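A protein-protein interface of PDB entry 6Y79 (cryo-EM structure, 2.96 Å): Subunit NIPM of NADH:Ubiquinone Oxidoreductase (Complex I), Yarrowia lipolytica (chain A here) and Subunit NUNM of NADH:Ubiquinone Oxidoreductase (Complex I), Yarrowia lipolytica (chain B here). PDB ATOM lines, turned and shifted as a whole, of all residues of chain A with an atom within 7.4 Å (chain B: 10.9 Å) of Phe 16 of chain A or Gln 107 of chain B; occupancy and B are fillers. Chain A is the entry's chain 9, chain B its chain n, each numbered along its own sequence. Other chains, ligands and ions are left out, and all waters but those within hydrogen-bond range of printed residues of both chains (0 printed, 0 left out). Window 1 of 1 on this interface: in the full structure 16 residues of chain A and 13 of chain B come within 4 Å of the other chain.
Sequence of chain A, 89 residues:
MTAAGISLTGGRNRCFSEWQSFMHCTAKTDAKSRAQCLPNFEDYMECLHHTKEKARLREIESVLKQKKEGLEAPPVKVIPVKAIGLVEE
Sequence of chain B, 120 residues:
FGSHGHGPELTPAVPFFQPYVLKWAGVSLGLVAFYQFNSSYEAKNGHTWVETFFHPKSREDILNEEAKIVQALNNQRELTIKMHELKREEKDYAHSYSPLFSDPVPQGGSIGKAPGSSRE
Of the 20 printed residues of chain B, 10 touch a printed residue of chain A.
Printed residues of chain B that touch a printed residue of chain A: Pro 104, Val 105, Pro 106, Gln 107, Gly 108, Gly 109, Gly 112, Ser 117, Ser 118 and Arg 119.
Printed residues of chain A that touch a printed residue of chain B: Gly 5, Ile 6, Gly 11, Arg 12, Phe 16, Ser 17, Trp 19, Gln 20, Ser 21 and Met 23.
Among the printed residues, 20 pairs touch across the chains.
The side-chain hydroxyl (OG) of Ser 117 of chain B is in hydrogen-bond range of the backbone carbonyl oxygen (O) of Ala 114 of chain B (2.8 Å).
The backbone carbonyl oxygen of Gly 5 of chain A sits at hydrogen-bond distance from the backbone NH of Asn 13 of chain A.
The side-chain amide oxygen (OD1) of Asn 13 of chain A lies within hydrogen-bond range of the backbone NH (N) of Phe 16 of chain A (3.1 Å).
The side-chain hydroxyl (OG) of Ser 21 of chain A sits at hydrogen-bond distance from the backbone carbonyl oxygen (O) of Glu 18 of chain A, at 2.6 Å.
The side-chain sulfur of Met 23 of chain A lies within hydrogen-bond range of the indole nitrogen of Trp 19 of chain A, 3.5 Å away.
SG of Cys 15 of chain A forms a disulfide with SG of Cys 47 of chain A, 2.0 Å away.
Among the printed residues, pairs that only touch across the chains: Ile 6 of chain A with Gly 109 of chain B, Gly 11 of chain A with Gly 109 of chain B, Gly 11 of chain A with Gly 112 of chain B, Arg 12 of chain A with Gly 108 of chain B, Phe 16 of chain A with Pro 106 of chain B, Phe 16 of chain A with Gln 107 of chain B, Phe 16 of chain A with Gly 108 of chain B, Phe 16 of chain A with Ser 117 of chain B, Ser 17 of chain A with Ser 118 of chain B, Ser 17 of chain A with Arg 119 of chain B, Trp 19 of chain A with Pro 106 of chain B, Gln 20 of chain A with Val 105 of chain B, Ser 21 of chain A with Arg 119 of chain B and Met 23 of chain A with Pro 104 of chain B.
O of Gly 109 of chain B lies within hydrogen-bond range of N of Arg 12 of chain A (3.5 Å).
OG of Ser 117 of chain B lies within hydrogen-bond range of NH1 of Arg 12 of chain A (2.5 Å).
The backbone carbonyl oxygen of Ser 117 of chain B lies within hydrogen-bond range of the side-chain hydroxyl of Ser 17 of chain A (2.6 Å).
The guanidinium group of Arg 12 of chain A is in hydrogen-bond range of the side-chain hydroxyl of Ser 118 of chain B, at 3.4 Å.
O of Ser 118 of chain B lies close to OE1 of Gln 20 of chain A.
O of Gly 5 of chain A lies close to O of Gly 108 of chain B (3.2 Å).
Phe 16 of chain A touches four residues of chain B.
Gln 107 of chain B touches one residue of chain A.
Gly 5 of chain A touches one residue of chain B.
No residue of chain B comes within 4 Å of Asn 13 of chain A.
No residue of chain B comes within 4 Å of Cys 15 of chain A.
Ser 17 of chain A touches just these residues of chain B: Ser 117 (2.6 Å), Ser 118 (3.7 Å) and Arg 119 (3.3 Å).
No residue of chain B comes within 4 Å of Glu 18 of chain A.
Of the printed residues of chain A, Val 105 of chain B touches Gln 20 (3.4 Å).
Of the printed residues of chain A, Arg 119 of chain B touches Ser 17 and Ser 21.
Printed residues of chain A within 4 Å of Pro 104 of chain B: Met 23 (3.4 Å).
Printed residues of chain A within 4 Å of Gly 109 of chain B: Ile 6 (3.7 Å), Gly 11 (3.2 Å) and Arg 12 (3.5 Å).
Printed residues of chain A within 4 Å of Ser 117 of chain B: Arg 12 (2.5 Å), Phe 16 (3.4 Å) and Ser 17 (2.6 Å).
The nearest residue of chain B that does not touch Phe 16 of chain A is Ser 118 of chain B (4.7 Å).
The nearest printed residue of chain A that does not touch Pro 104 of chain B is Trp 19 of chain A (5.7 Å).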
ATOM      1  N   ALA A   4      -5.941  -1.524  31.253  1.00  0.00           N
ATOM      2  CA  ALA A   4      -6.223  -0.950  29.941  1.00  0.00           C
ATOM      3  C   ALA A   4      -5.687   0.471  29.832  1.00  0.00           C
ATOM      4  O   ALA A   4      -4.944   0.796  28.900  1.00  0.00           O
ATOM      5  CB  ALA A   4      -7.723  -0.991  29.663  1.00  0.00           C
ATOM      6  N   GLY A   5      -6.028   1.329  30.782  1.00  0.00           N
ATOM      7  CA  GLY A   5      -5.572   2.699  30.697  1.00  0.00           C
ATOM      8  C   GLY A   5      -4.756   3.158  31.882  1.00  0.00           C
ATOM      9  O   GLY A   5      -4.741   4.345  32.191  1.00  0.00           O
ATOM     10  N   ILE A   6      -4.075   2.242  32.551  1.00  0.00           N
ATOM     11  CA  ILE A   6      -3.309   2.564  33.746  1.00  0.00           C
ATOM     12  C   ILE A   6      -1.908   2.974  33.326  1.00  0.00           C
ATOM     13  O   ILE A   6      -1.260   2.275  32.544  1.00  0.00           O
ATOM     14  CB  ILE A   6      -3.276   1.370  34.712  1.00  0.00           C
ATOM     15  CG1 ILE A   6      -4.700   0.883  34.977  1.00  0.00           C
ATOM     16  CG2 ILE A   6      -2.595   1.750  36.003  1.00  0.00           C
ATOM     17  CD1 ILE A   6      -4.785  -0.325  35.858  1.00  0.00           C
ATOM     18  N   GLY A  11      -2.025   6.469  37.190  1.00  0.00           N
ATOM     19  CA  GLY A  11      -3.025   7.336  36.613  1.00  0.00           C
ATOM     20  C   GLY A  11      -3.447   6.850  35.245  1.00  0.00           C
ATOM     21  O   GLY A  11      -3.274   5.685  34.887  1.00  0.00           O
ATOM     22  N   ARG A  12      -4.012   7.759  34.468  1.00  0.00           N
ATOM     23  CA  ARG A  12      -4.390   7.442  33.102  1.00  0.00           C
ATOM     24  C   ARG A  12      -3.206   7.686  32.173  1.00  0.00           C
ATOM     25  O   ARG A  12      -2.359   8.540  32.437  1.00  0.00           O
ATOM     26  CB  ARG A  12      -5.610   8.262  32.686  1.00  0.00           C
ATOM     27  CG  ARG A  12      -6.831   7.969  33.540  1.00  0.00           C
ATOM     28  CD  ARG A  12      -7.850   9.058  33.488  1.00  0.00           C
ATOM     29  NE  ARG A  12      -9.122   8.655  34.067  1.00  0.00           N
ATOM     30  CZ  ARG A  12     -10.298   9.172  33.735  1.00  0.00           C
ATOM     31  NH1 ARG A  12     -10.362  10.116  32.823  1.00  0.00           N
ATOM     32  NH2 ARG A  12     -11.412   8.741  34.316  1.00  0.00           N
ATOM     33  N   ASN A  13      -3.127   6.909  31.093  1.00  0.00           N
ATOM     34  CA  ASN A  13      -1.943   6.983  30.245  1.00  0.00           C
ATOM     35  C   ASN A  13      -2.031   8.202  29.329  1.00  0.00           C
ATOM     36  O   ASN A  13      -2.925   9.043  29.447  1.00  0.00           O
ATOM     37  CB  ASN A  13      -1.703   5.665  29.497  1.00  0.00           C
ATOM     38  CG  ASN A  13      -2.877   5.182  28.695  1.00  0.00           C
ATOM     39  OD1 ASN A  13      -3.823   5.895  28.451  1.00  0.00           O
ATOM     40  ND2 ASN A  13      -2.797   3.941  28.252  1.00  0.00           N
ATOM     41  N   ARG A  14      -1.074   8.319  28.413  1.00  0.00           N
ATOM     42  CA  ARG A  14      -0.969   9.522  27.601  1.00  0.00           C
ATOM     43  C   ARG A  14      -2.089   9.614  26.575  1.00  0.00           C
ATOM     44  O   ARG A  14      -2.573  10.712  26.283  1.00  0.00           O
ATOM     45  CB  ARG A  14       0.387   9.548  26.915  1.00  0.00           C
ATOM     46  CG  ARG A  14       0.742  10.856  26.291  1.00  0.00           C
ATOM     47  CD  ARG A  14       2.035  10.705  25.554  1.00  0.00           C
ATOM     48  NE  ARG A  14       1.931   9.666  24.542  1.00  0.00           N
ATOM     49  CZ  ARG A  14       2.971   9.157  23.901  1.00  0.00           C
ATOM     50  NH1 ARG A  14       2.794   8.214  22.994  1.00  0.00           N
ATOM     51  NH2 ARG A  14       4.193   9.593  24.175  1.00  0.00           N
ATOM     52  N   CYS A  15      -2.530   8.484  26.036  1.00  0.00           N
ATOM     53  CA  CYS A  15      -3.584   8.459  25.034  1.00  0.00           C
ATOM     54  C   CYS A  15      -4.890   7.924  25.590  1.00  0.00           C
ATOM     55  O   CYS A  15      -5.655   7.284  24.869  1.00  0.00           O
ATOM     56  CB  CYS A  15      -3.165   7.625  23.835  1.00  0.00           C
ATOM     57  SG  CYS A  15      -1.818   8.330  22.936  1.00  0.00           S
ATOM     58  N   PHE A  16      -5.146   8.158  26.873  1.00  0.00           N
ATOM     59  CA  PHE A  16      -6.386   7.677  27.459  1.00  0.00           C
ATOM     60  C   PHE A  16      -7.583   8.435  26.933  1.00  0.00           C
ATOM     61  O   PHE A  16      -8.660   7.852  26.773  1.00  0.00           O
ATOM     62  CB  PHE A  16      -6.351   7.790  28.974  1.00  0.00           C
ATOM     63  CG  PHE A  16      -7.557   7.232  29.628  1.00  0.00           C
ATOM     64  CD1 PHE A  16      -7.743   5.869  29.690  1.00  0.00           C
ATOM     65  CD2 PHE A  16      -8.519   8.062  30.152  1.00  0.00           C
ATOM     66  CE1 PHE A  16      -8.852   5.347  30.279  1.00  0.00           C
ATOM     67  CE2 PHE A  16      -9.621   7.537  30.749  1.00  0.00           C
ATOM     68  CZ  PHE A  16      -9.791   6.184  30.804  1.00  0.00           C
ATOM     69  N   SER A  17      -7.431   9.734  26.689  1.00  0.00           N
ATOM     70  CA  SER A  17      -8.615  10.523  26.408  1.00  0.00           C
ATOM     71  C   SER A  17      -9.086  10.285  24.980  1.00  0.00           C
ATOM     72  O   SER A  17     -10.289  10.183  24.727  1.00  0.00           O
ATOM     73  CB  SER A  17      -8.328  11.990  26.692  1.00  0.00           C
ATOM     74  OG  SER A  17      -7.770  12.155  27.982  1.00  0.00           O
ATOM     75  N   GLU A  18      -8.148  10.142  24.046  1.00  0.00           N
ATOM     76  CA  GLU A  18      -8.484   9.782  22.672  1.00  0.00           C
ATOM     77  C   GLU A  18      -9.087   8.387  22.599  1.00  0.00           C
ATOM     78  O   GLU A  18     -10.042   8.158  21.848  1.00  0.00           O
ATOM     79  CB  GLU A  18      -7.233   9.879  21.799  1.00  0.00           C
ATOM     80  CG  GLU A  18      -6.729  11.293  21.598  1.00  0.00           C
ATOM     81  CD  GLU A  18      -5.783  11.776  22.695  1.00  0.00           C
ATOM     82  OE1 GLU A  18      -5.756  11.190  23.797  1.00  0.00           O
ATOM     83  OE2 GLU A  18      -5.067  12.769  22.456  1.00  0.00           O
ATOM     84  N   TRP A  19      -8.568   7.452  23.402  1.00  0.00           N
ATOM     85  CA  TRP A  19      -9.138   6.114  23.449  1.00  0.00           C
ATOM     86  C   TRP A  19     -10.531   6.120  24.051  1.00  0.00           C
ATOM     87  O   TRP A  19     -11.407   5.397  23.578  1.00  0.00           O
ATOM     88  CB  TRP A  19      -8.244   5.171  24.242  1.00  0.00           C
ATOM     89  CG  TRP A  19      -8.732   3.766  24.162  1.00  0.00           C
ATOM     90  CD1 TRP A  19      -9.223   3.140  23.061  1.00  0.00           C
ATOM     91  CD2 TRP A  19      -8.798   2.816  25.224  1.00  0.00           C
ATOM     92  NE1 TRP A  19      -9.589   1.860  23.364  1.00  0.00           N
ATOM     93  CE2 TRP A  19      -9.338   1.633  24.689  1.00  0.00           C
ATOM     94  CE3 TRP A  19      -8.453   2.848  26.577  1.00  0.00           C
ATOM     95  CZ2 TRP A  19      -9.542   0.494  25.456  1.00  0.00           C
ATOM     96  CZ3 TRP A  19      -8.644   1.714  27.332  1.00  0.00           C
ATOM     97  CH2 TRP A  19      -9.193   0.555  26.774  1.00  0.00           C
ATOM     98  N   GLN A  20     -10.762   6.924  25.089  1.00  0.00           N
ATOM     99  CA  GLN A  20     -12.085   6.950  25.699  1.00  0.00           C
ATOM    100  C   GLN A  20     -13.093   7.643  24.795  1.00  0.00           C
ATOM    101  O   GLN A  20     -14.272   7.279  24.794  1.00  0.00           O
ATOM    102  CB  GLN A  20     -12.034   7.614  27.075  1.00  0.00           C
ATOM    103  CG  GLN A  20     -13.240   7.274  27.942  1.00  0.00           C
ATOM    104  CD  GLN A  20     -13.303   8.047  29.244  1.00  0.00           C
ATOM    105  OE1 GLN A  20     -12.317   8.598  29.694  1.00  0.00           O
ATOM    106  NE2 GLN A  20     -14.479   8.095  29.849  1.00  0.00           N
ATOM    107  N   SER A  21     -12.641   8.600  23.984  1.00  0.00           N
ATOM    108  CA  SER A  21     -13.513   9.177  22.968  1.00  0.00           C
ATOM    109  C   SER A  21     -13.853   8.159  21.886  1.00  0.00           C
ATOM    110  O   SER A  21     -15.000   8.092  21.427  1.00  0.00           O
ATOM    111  CB  SER A  21     -12.854  10.407  22.356  1.00  0.00           C
ATOM    112  OG  SER A  21     -11.844  10.029  21.443  1.00  0.00           O
ATOM    113  N   PHE A  22     -12.865   7.353  21.474  1.00  0.00           N
ATOM    114  CA  PHE A  22     -13.120   6.288  20.512  1.00  0.00           C
ATOM    115  C   PHE A  22     -14.061   5.231  21.074  1.00  0.00           C
ATOM    116  O   PHE A  22     -14.911   4.724  20.355  1.00  0.00           O
ATOM    117  CB  PHE A  22     -11.813   5.633  20.075  1.00  0.00           C
ATOM    118  CG  PHE A  22     -12.005   4.527  19.084  1.00  0.00           C
ATOM    119  CD1 PHE A  22     -12.489   4.801  17.819  1.00  0.00           C
ATOM    120  CD2 PHE A  22     -11.717   3.213  19.417  1.00  0.00           C
ATOM    121  CE1 PHE A  22     -12.686   3.788  16.903  1.00  0.00           C
ATOM    122  CE2 PHE A  22     -11.909   2.196  18.504  1.00  0.00           C
ATOM    123  CZ  PHE A  22     -12.390   2.486  17.246  1.00  0.00           C
ATOM    124  N   MET A  23     -13.945   4.897  22.349  1.00  0.00           N
ATOM    125  CA  MET A  23     -14.875   3.944  22.946  1.00  0.00           C
ATOM    126  C   MET A  23     -16.264   4.539  23.177  1.00  0.00           C
ATOM    127  O   MET A  23     -17.253   3.798  23.182  1.00  0.00           O
ATOM    128  CB  MET A  23     -14.306   3.416  24.256  1.00  0.00           C
ATOM    129  CG  MET A  23     -13.003   2.653  24.109  1.00  0.00           C
ATOM    130  SD  MET A  23     -13.061   1.327  22.902  1.00  0.00           S
ATOM    131  CE  MET A  23     -13.717   0.007  23.907  1.00  0.00           C
ATOM    132  N   TYR A  44      -6.718   8.536  17.690  1.00  0.00           N
ATOM    133  CA  TYR A  44      -6.056   7.675  18.649  1.00  0.00           C
ATOM    134  C   TYR A  44      -4.712   7.218  18.118  1.00  0.00           C
ATOM    135  O   TYR A  44      -3.711   7.267  18.842  1.00  0.00           O
ATOM    136  CB  TYR A  44      -6.931   6.479  18.977  1.00  0.00           C
ATOM    137  CG  TYR A  44      -6.294   5.596  19.998  1.00  0.00           C
ATOM    138  CD1 TYR A  44      -5.963   6.093  21.244  1.00  0.00           C
ATOM    139  CD2 TYR A  44      -6.003   4.272  19.718  1.00  0.00           C
ATOM    140  CE1 TYR A  44      -5.368   5.300  22.183  1.00  0.00           C
ATOM    141  CE2 TYR A  44      -5.410   3.471  20.655  1.00  0.00           C
ATOM    142  CZ  TYR A  44      -5.099   3.993  21.888  1.00  0.00           C
ATOM    143  OH  TYR A  44      -4.513   3.210  22.841  1.00  0.00           O
ATOM    144  N   CYS A  47      -2.192   9.739  18.060  1.00  0.00           N
ATOM    145  CA  CYS A  47      -1.801   9.963  19.451  1.00  0.00           C
ATOM    146  C   CYS A  47      -0.691   9.013  19.847  1.00  0.00           C
ATOM    147  O   CYS A  47       0.238   9.397  20.560  1.00  0.00           O
ATOM    148  CB  CYS A  47      -2.974   9.775  20.411  1.00  0.00           C
ATOM    149  SG  CYS A  47      -2.562  10.070  22.184  1.00  0.00           S
ATOM    150  N   TYR B  93     -23.125  -5.686  22.758  1.00  0.00           N
ATOM    151  CA  TYR B  93     -21.976  -5.819  23.647  1.00  0.00           C
ATOM    152  C   TYR B  93     -22.345  -6.546  24.929  1.00  0.00           C
ATOM    153  O   TYR B  93     -21.500  -7.229  25.514  1.00  0.00           O
ATOM    154  CB  TYR B  93     -21.416  -4.436  23.952  1.00  0.00           C
ATOM    155  CG  TYR B  93     -20.194  -4.377  24.838  1.00  0.00           C
ATOM    156  CD1 TYR B  93     -18.922  -4.530  24.316  1.00  0.00           C
ATOM    157  CD2 TYR B  93     -20.315  -4.123  26.196  1.00  0.00           C
ATOM    158  CE1 TYR B  93     -17.815  -4.452  25.121  1.00  0.00           C
ATOM    159  CE2 TYR B  93     -19.212  -4.043  27.005  1.00  0.00           C
ATOM    160  CZ  TYR B  93     -17.965  -4.200  26.460  1.00  0.00           C
ATOM    161  OH  TYR B  93     -16.859  -4.128  27.272  1.00  0.00           O
ATOM    162  N   PHE B 101     -21.516  -4.933  33.565  1.00  0.00           N
ATOM    163  CA  PHE B 101     -20.595  -3.954  32.977  1.00  0.00           C
ATOM    164  C   PHE B 101     -20.753  -3.895  31.457  1.00  0.00           C
ATOM    165  O   PHE B 101     -19.859  -4.237  30.686  1.00  0.00           O
ATOM    166  CB  PHE B 101     -19.137  -4.229  33.352  1.00  0.00           C
ATOM    167  CG  PHE B 101     -18.856  -4.049  34.779  1.00  0.00           C
ATOM    168  CD1 PHE B 101     -18.586  -2.788  35.266  1.00  0.00           C
ATOM    169  CD2 PHE B 101     -18.874  -5.122  35.645  1.00  0.00           C
ATOM    170  CE1 PHE B 101     -18.329  -2.596  36.584  1.00  0.00           C
ATOM    171  CE2 PHE B 101     -18.619  -4.935  36.969  1.00  0.00           C
ATOM    172  CZ  PHE B 101     -18.332  -3.670  37.427  1.00  0.00           C
ATOM    173  N   SER B 102     -21.929  -3.428  31.054  1.00  0.00           N
ATOM    174  CA  SER B 102     -22.274  -3.327  29.646  1.00  0.00           C
ATOM    175  C   SER B 102     -21.695  -2.099  28.954  1.00  0.00           C
ATOM    176  O   SER B 102     -21.990  -1.900  27.770  1.00  0.00           O
ATOM    177  CB  SER B 102     -23.792  -3.329  29.484  1.00  0.00           C
ATOM    178  OG  SER B 102     -24.339  -4.560  29.904  1.00  0.00           O
ATOM    179  N   ASP B 103     -20.848  -1.198  29.695  1.00  0.00           N
ATOM    180  CA  ASP B 103     -20.385  -0.195  28.748  1.00  0.00           C
ATOM    181  C   ASP B 103     -18.920  -0.416  28.381  1.00  0.00           C
ATOM    182  O   ASP B 103     -18.106  -0.796  29.228  1.00  0.00           O
ATOM    183  CB  ASP B 103     -20.586   1.221  29.294  1.00  0.00           C
ATOM    184  CG  ASP B 103     -19.810   1.497  30.563  1.00  0.00           C
ATOM    185  OD1 ASP B 103     -19.525   0.553  31.330  1.00  0.00           O
ATOM    186  OD2 ASP B 103     -19.479   2.681  30.786  1.00  0.00           O
ATOM    187  N   PRO B 104     -18.562  -0.206  27.112  1.00  0.00           N
ATOM    188  CA  PRO B 104     -17.160  -0.363  26.700  1.00  0.00           C
ATOM    189  C   PRO B 104     -16.227   0.730  27.197  1.00  0.00           C
ATOM    190  O   PRO B 104     -15.016   0.630  26.962  1.00  0.00           O
ATOM    191  CB  PRO B 104     -17.243  -0.342  25.164  1.00  0.00           C
ATOM    192  CG  PRO B 104     -18.652  -0.677  24.847  1.00  0.00           C
ATOM    193  CD  PRO B 104     -19.466  -0.099  25.956  1.00  0.00           C
ATOM    194  N   VAL B 105     -16.742   1.761  27.856  1.00  0.00           N
ATOM    195  CA  VAL B 105     -15.953   2.900  28.316  1.00  0.00           C
ATOM    196  C   VAL B 105     -15.031   2.470  29.453  1.00  0.00           C
ATOM    197  O   VAL B 105     -15.502   1.974  30.487  1.00  0.00           O
ATOM    198  CB  VAL B 105     -16.874   4.052  28.732  1.00  0.00           C
ATOM    199  CG1 VAL B 105     -16.068   5.223  29.175  1.00  0.00           C
ATOM    200  CG2 VAL B 105     -17.763   4.435  27.572  1.00  0.00           C
ATOM    201  N   PRO B 106     -13.717   2.647  29.298  1.00  0.00           N
ATOM    202  CA  PRO B 106     -12.771   2.005  30.229  1.00  0.00           C
ATOM    203  C   PRO B 106     -12.672   2.645  31.603  1.00  0.00           C
ATOM    204  O   PRO B 106     -12.641   1.917  32.605  1.00  0.00           O
ATOM    205  CB  PRO B 106     -11.446   2.110  29.476  1.00  0.00           C
ATOM    206  CG  PRO B 106     -11.632   3.243  28.537  1.00  0.00           C
ATOM    207  CD  PRO B 106     -13.039   3.167  28.103  1.00  0.00           C
ATOM    208  N   GLN B 107     -12.626   3.982  31.660  1.00  0.00           N
ATOM    209  CA  GLN B 107     -12.355   4.834  32.843  1.00  0.00           C
ATOM    210  C   GLN B 107     -11.288   4.251  33.777  1.00  0.00           C
ATOM    211  O   GLN B 107     -11.425   4.238  35.001  1.00  0.00           O
ATOM    212  CB  GLN B 107     -13.643   5.189  33.607  1.00  0.00           C
ATOM    213  CG  GLN B 107     -14.478   4.055  34.113  1.00  0.00           C
ATOM    214  CD  GLN B 107     -15.539   4.521  35.052  1.00  0.00           C
ATOM    215  OE1 GLN B 107     -16.129   5.591  34.864  1.00  0.00           O
ATOM    216  NE2 GLN B 107     -15.740   3.756  36.137  1.00  0.00           N
ATOM    217  N   GLY B 108     -10.185   3.798  33.188  1.00  0.00           N
ATOM    218  CA  GLY B 108      -9.205   2.998  33.899  1.00  0.00           C
ATOM    219  C   GLY B 108      -7.990   3.809  34.311  1.00  0.00           C
ATOM    220  O   GLY B 108      -7.571   4.722  33.603  1.00  0.00           O
ATOM    221  N   GLY B 109      -7.415   3.435  35.447  1.00  0.00           N
ATOM    222  CA  GLY B 109      -6.232   4.105  35.953  1.00  0.00           C
ATOM    223  C   GLY B 109      -6.527   5.175  36.986  1.00  0.00           C
ATOM    224  O   GLY B 109      -6.185   6.344  36.802  1.00  0.00           O
ATOM    225  N   SER B 110      -7.215   4.812  38.064  1.00  0.00           N
ATOM    226  CA  SER B 110      -7.754   5.820  38.969  1.00  0.00           C
ATOM    227  C   SER B 110      -6.960   5.972  40.267  1.00  0.00           C
ATOM    228  O   SER B 110      -7.468   5.674  41.347  1.00  0.00           O
ATOM    229  CB  SER B 110      -9.208   5.499  39.259  1.00  0.00           C
ATOM    230  OG  SER B 110      -9.765   6.462  40.130  1.00  0.00           O
ATOM    231  N   ILE B 111      -5.724   6.512  40.177  1.00  0.00           N
ATOM    232  CA  ILE B 111      -5.124   7.123  41.368  1.00  0.00           C
ATOM    233  C   ILE B 111      -4.587   8.526  41.057  1.00  0.00           C
ATOM    234  O   ILE B 111      -5.011   9.489  41.690  1.00  0.00           O
ATOM    235  CB  ILE B 111      -4.048   6.246  42.076  1.00  0.00           C
ATOM    236  CG1 ILE B 111      -2.810   5.878  41.254  1.00  0.00           C
ATOM    237  CG2 ILE B 111      -4.614   4.950  42.660  1.00  0.00           C
ATOM    238  CD1 ILE B 111      -1.752   5.261  42.110  1.00  0.00           C
ATOM    239  N   GLY B 112      -3.687   8.694  40.092  1.00  0.00           N
ATOM    240  CA  GLY B 112      -3.026   9.982  39.965  1.00  0.00           C
ATOM    241  C   GLY B 112      -3.652  10.803  38.865  1.00  0.00           C
ATOM    242  O   GLY B 112      -2.962  11.485  38.103  1.00  0.00           O
ATOM    243  N   LYS B 113      -4.974  10.738  38.783  1.00  0.00           N
ATOM    244  CA  LYS B 113      -5.666  11.106  37.563  1.00  0.00           C
ATOM    245  C   LYS B 113      -5.842  12.613  37.470  1.00  0.00           C
ATOM    246  O   LYS B 113      -5.968  13.312  38.479  1.00  0.00           O
ATOM    247  CB  LYS B 113      -7.004  10.363  37.479  1.00  0.00           C
ATOM    248  CG  LYS B 113      -8.245  11.148  37.799  1.00  0.00           C
ATOM    249  CD  LYS B 113      -9.456  10.245  37.789  1.00  0.00           C
ATOM    250  CE  LYS B 113     -10.723  11.043  37.997  1.00  0.00           C
ATOM    251  NZ  LYS B 113     -11.926  10.178  38.035  1.00  0.00           N
ATOM    252  N   ALA B 114      -5.788  13.101  36.259  1.00  0.00           N
ATOM    253  CA  ALA B 114      -5.896  14.497  35.873  1.00  0.00           C
ATOM    254  C   ALA B 114      -7.344  14.823  35.559  1.00  0.00           C
ATOM    255  O   ALA B 114      -8.029  14.006  34.941  1.00  0.00           O
ATOM    256  CB  ALA B 114      -5.030  14.776  34.655  1.00  0.00           C
ATOM    257  N   PRO B 115      -7.881  15.949  36.019  1.00  0.00           N
ATOM    258  CA  PRO B 115      -9.150  16.418  35.449  1.00  0.00           C
ATOM    259  C   PRO B 115      -8.948  16.988  34.053  1.00  0.00           C
ATOM    260  O   PRO B 115      -7.977  17.697  33.785  1.00  0.00           O
ATOM    261  CB  PRO B 115      -9.618  17.474  36.452  1.00  0.00           C
ATOM    262  CG  PRO B 115      -9.040  16.984  37.740  1.00  0.00           C
ATOM    263  CD  PRO B 115      -7.669  16.506  37.365  1.00  0.00           C
ATOM    264  N   GLY B 116      -9.876  16.660  33.157  1.00  0.00           N
ATOM    265  CA  GLY B 116      -9.699  16.896  31.745  1.00  0.00           C
ATOM    266  C   GLY B 116      -9.230  15.689  30.967  1.00  0.00           C
ATOM    267  O   GLY B 116      -8.863  15.829  29.788  1.00  0.00           O
ATOM    268  N   SER B 117      -9.235  14.509  31.585  1.00  0.00           N
ATOM    269  CA  SER B 117      -8.665  13.317  30.989  1.00  0.00           C
ATOM    270  C   SER B 117      -9.715  12.426  30.347  1.00  0.00           C
ATOM    271  O   SER B 117      -9.393  11.322  29.901  1.00  0.00           O
ATOM    272  CB  SER B 117      -7.893  12.539  32.040  1.00  0.00           C
ATOM    273  OG  SER B 117      -8.798  12.111  33.049  1.00  0.00           O
ATOM    274  N   SER B 118     -10.959  12.881  30.271  1.00  0.00           N
ATOM    275  CA  SER B 118     -12.065  11.961  30.008  1.00  0.00           C
ATOM    276  C   SER B 118     -12.371  11.835  28.516  1.00  0.00           C
ATOM    277  O   SER B 118     -12.136  10.777  27.925  1.00  0.00           O
ATOM    278  CB  SER B 118     -13.289  12.406  30.806  1.00  0.00           C
ATOM    279  OG  SER B 118     -13.118  12.082  32.172  1.00  0.00           O
ATOM    280  N   ARG B 119     -12.804  12.931  27.889  1.00  0.00           N
ATOM    281  CA  ARG B 119     -13.470  12.911  26.569  1.00  0.00           C
ATOM    282  C   ARG B 119     -14.573  11.853  26.493  1.00  0.00           C
ATOM    283  O   ARG B 119     -15.305  11.773  25.511  1.00  0.00           O
ATOM    284  CB  ARG B 119     -12.465  12.705  25.437  1.00  0.00           C
ATOM    285  CG  ARG B 119     -11.563  13.880  25.147  1.00  0.00           C
ATOM    286  CD  ARG B 119     -10.521  13.458  24.137  1.00  0.00           C
ATOM    287  NE  ARG B 119      -9.936  14.573  23.433  1.00  0.00           N
ATOM    288  CZ  ARG B 119      -8.741  15.082  23.682  1.00  0.00           C
ATOM    289  NH1 ARG B 119      -7.965  14.581  24.628  1.00  0.00           N
ATOM    290  NH2 ARG B 119      -8.332  16.108  22.970  1.00  0.00           N
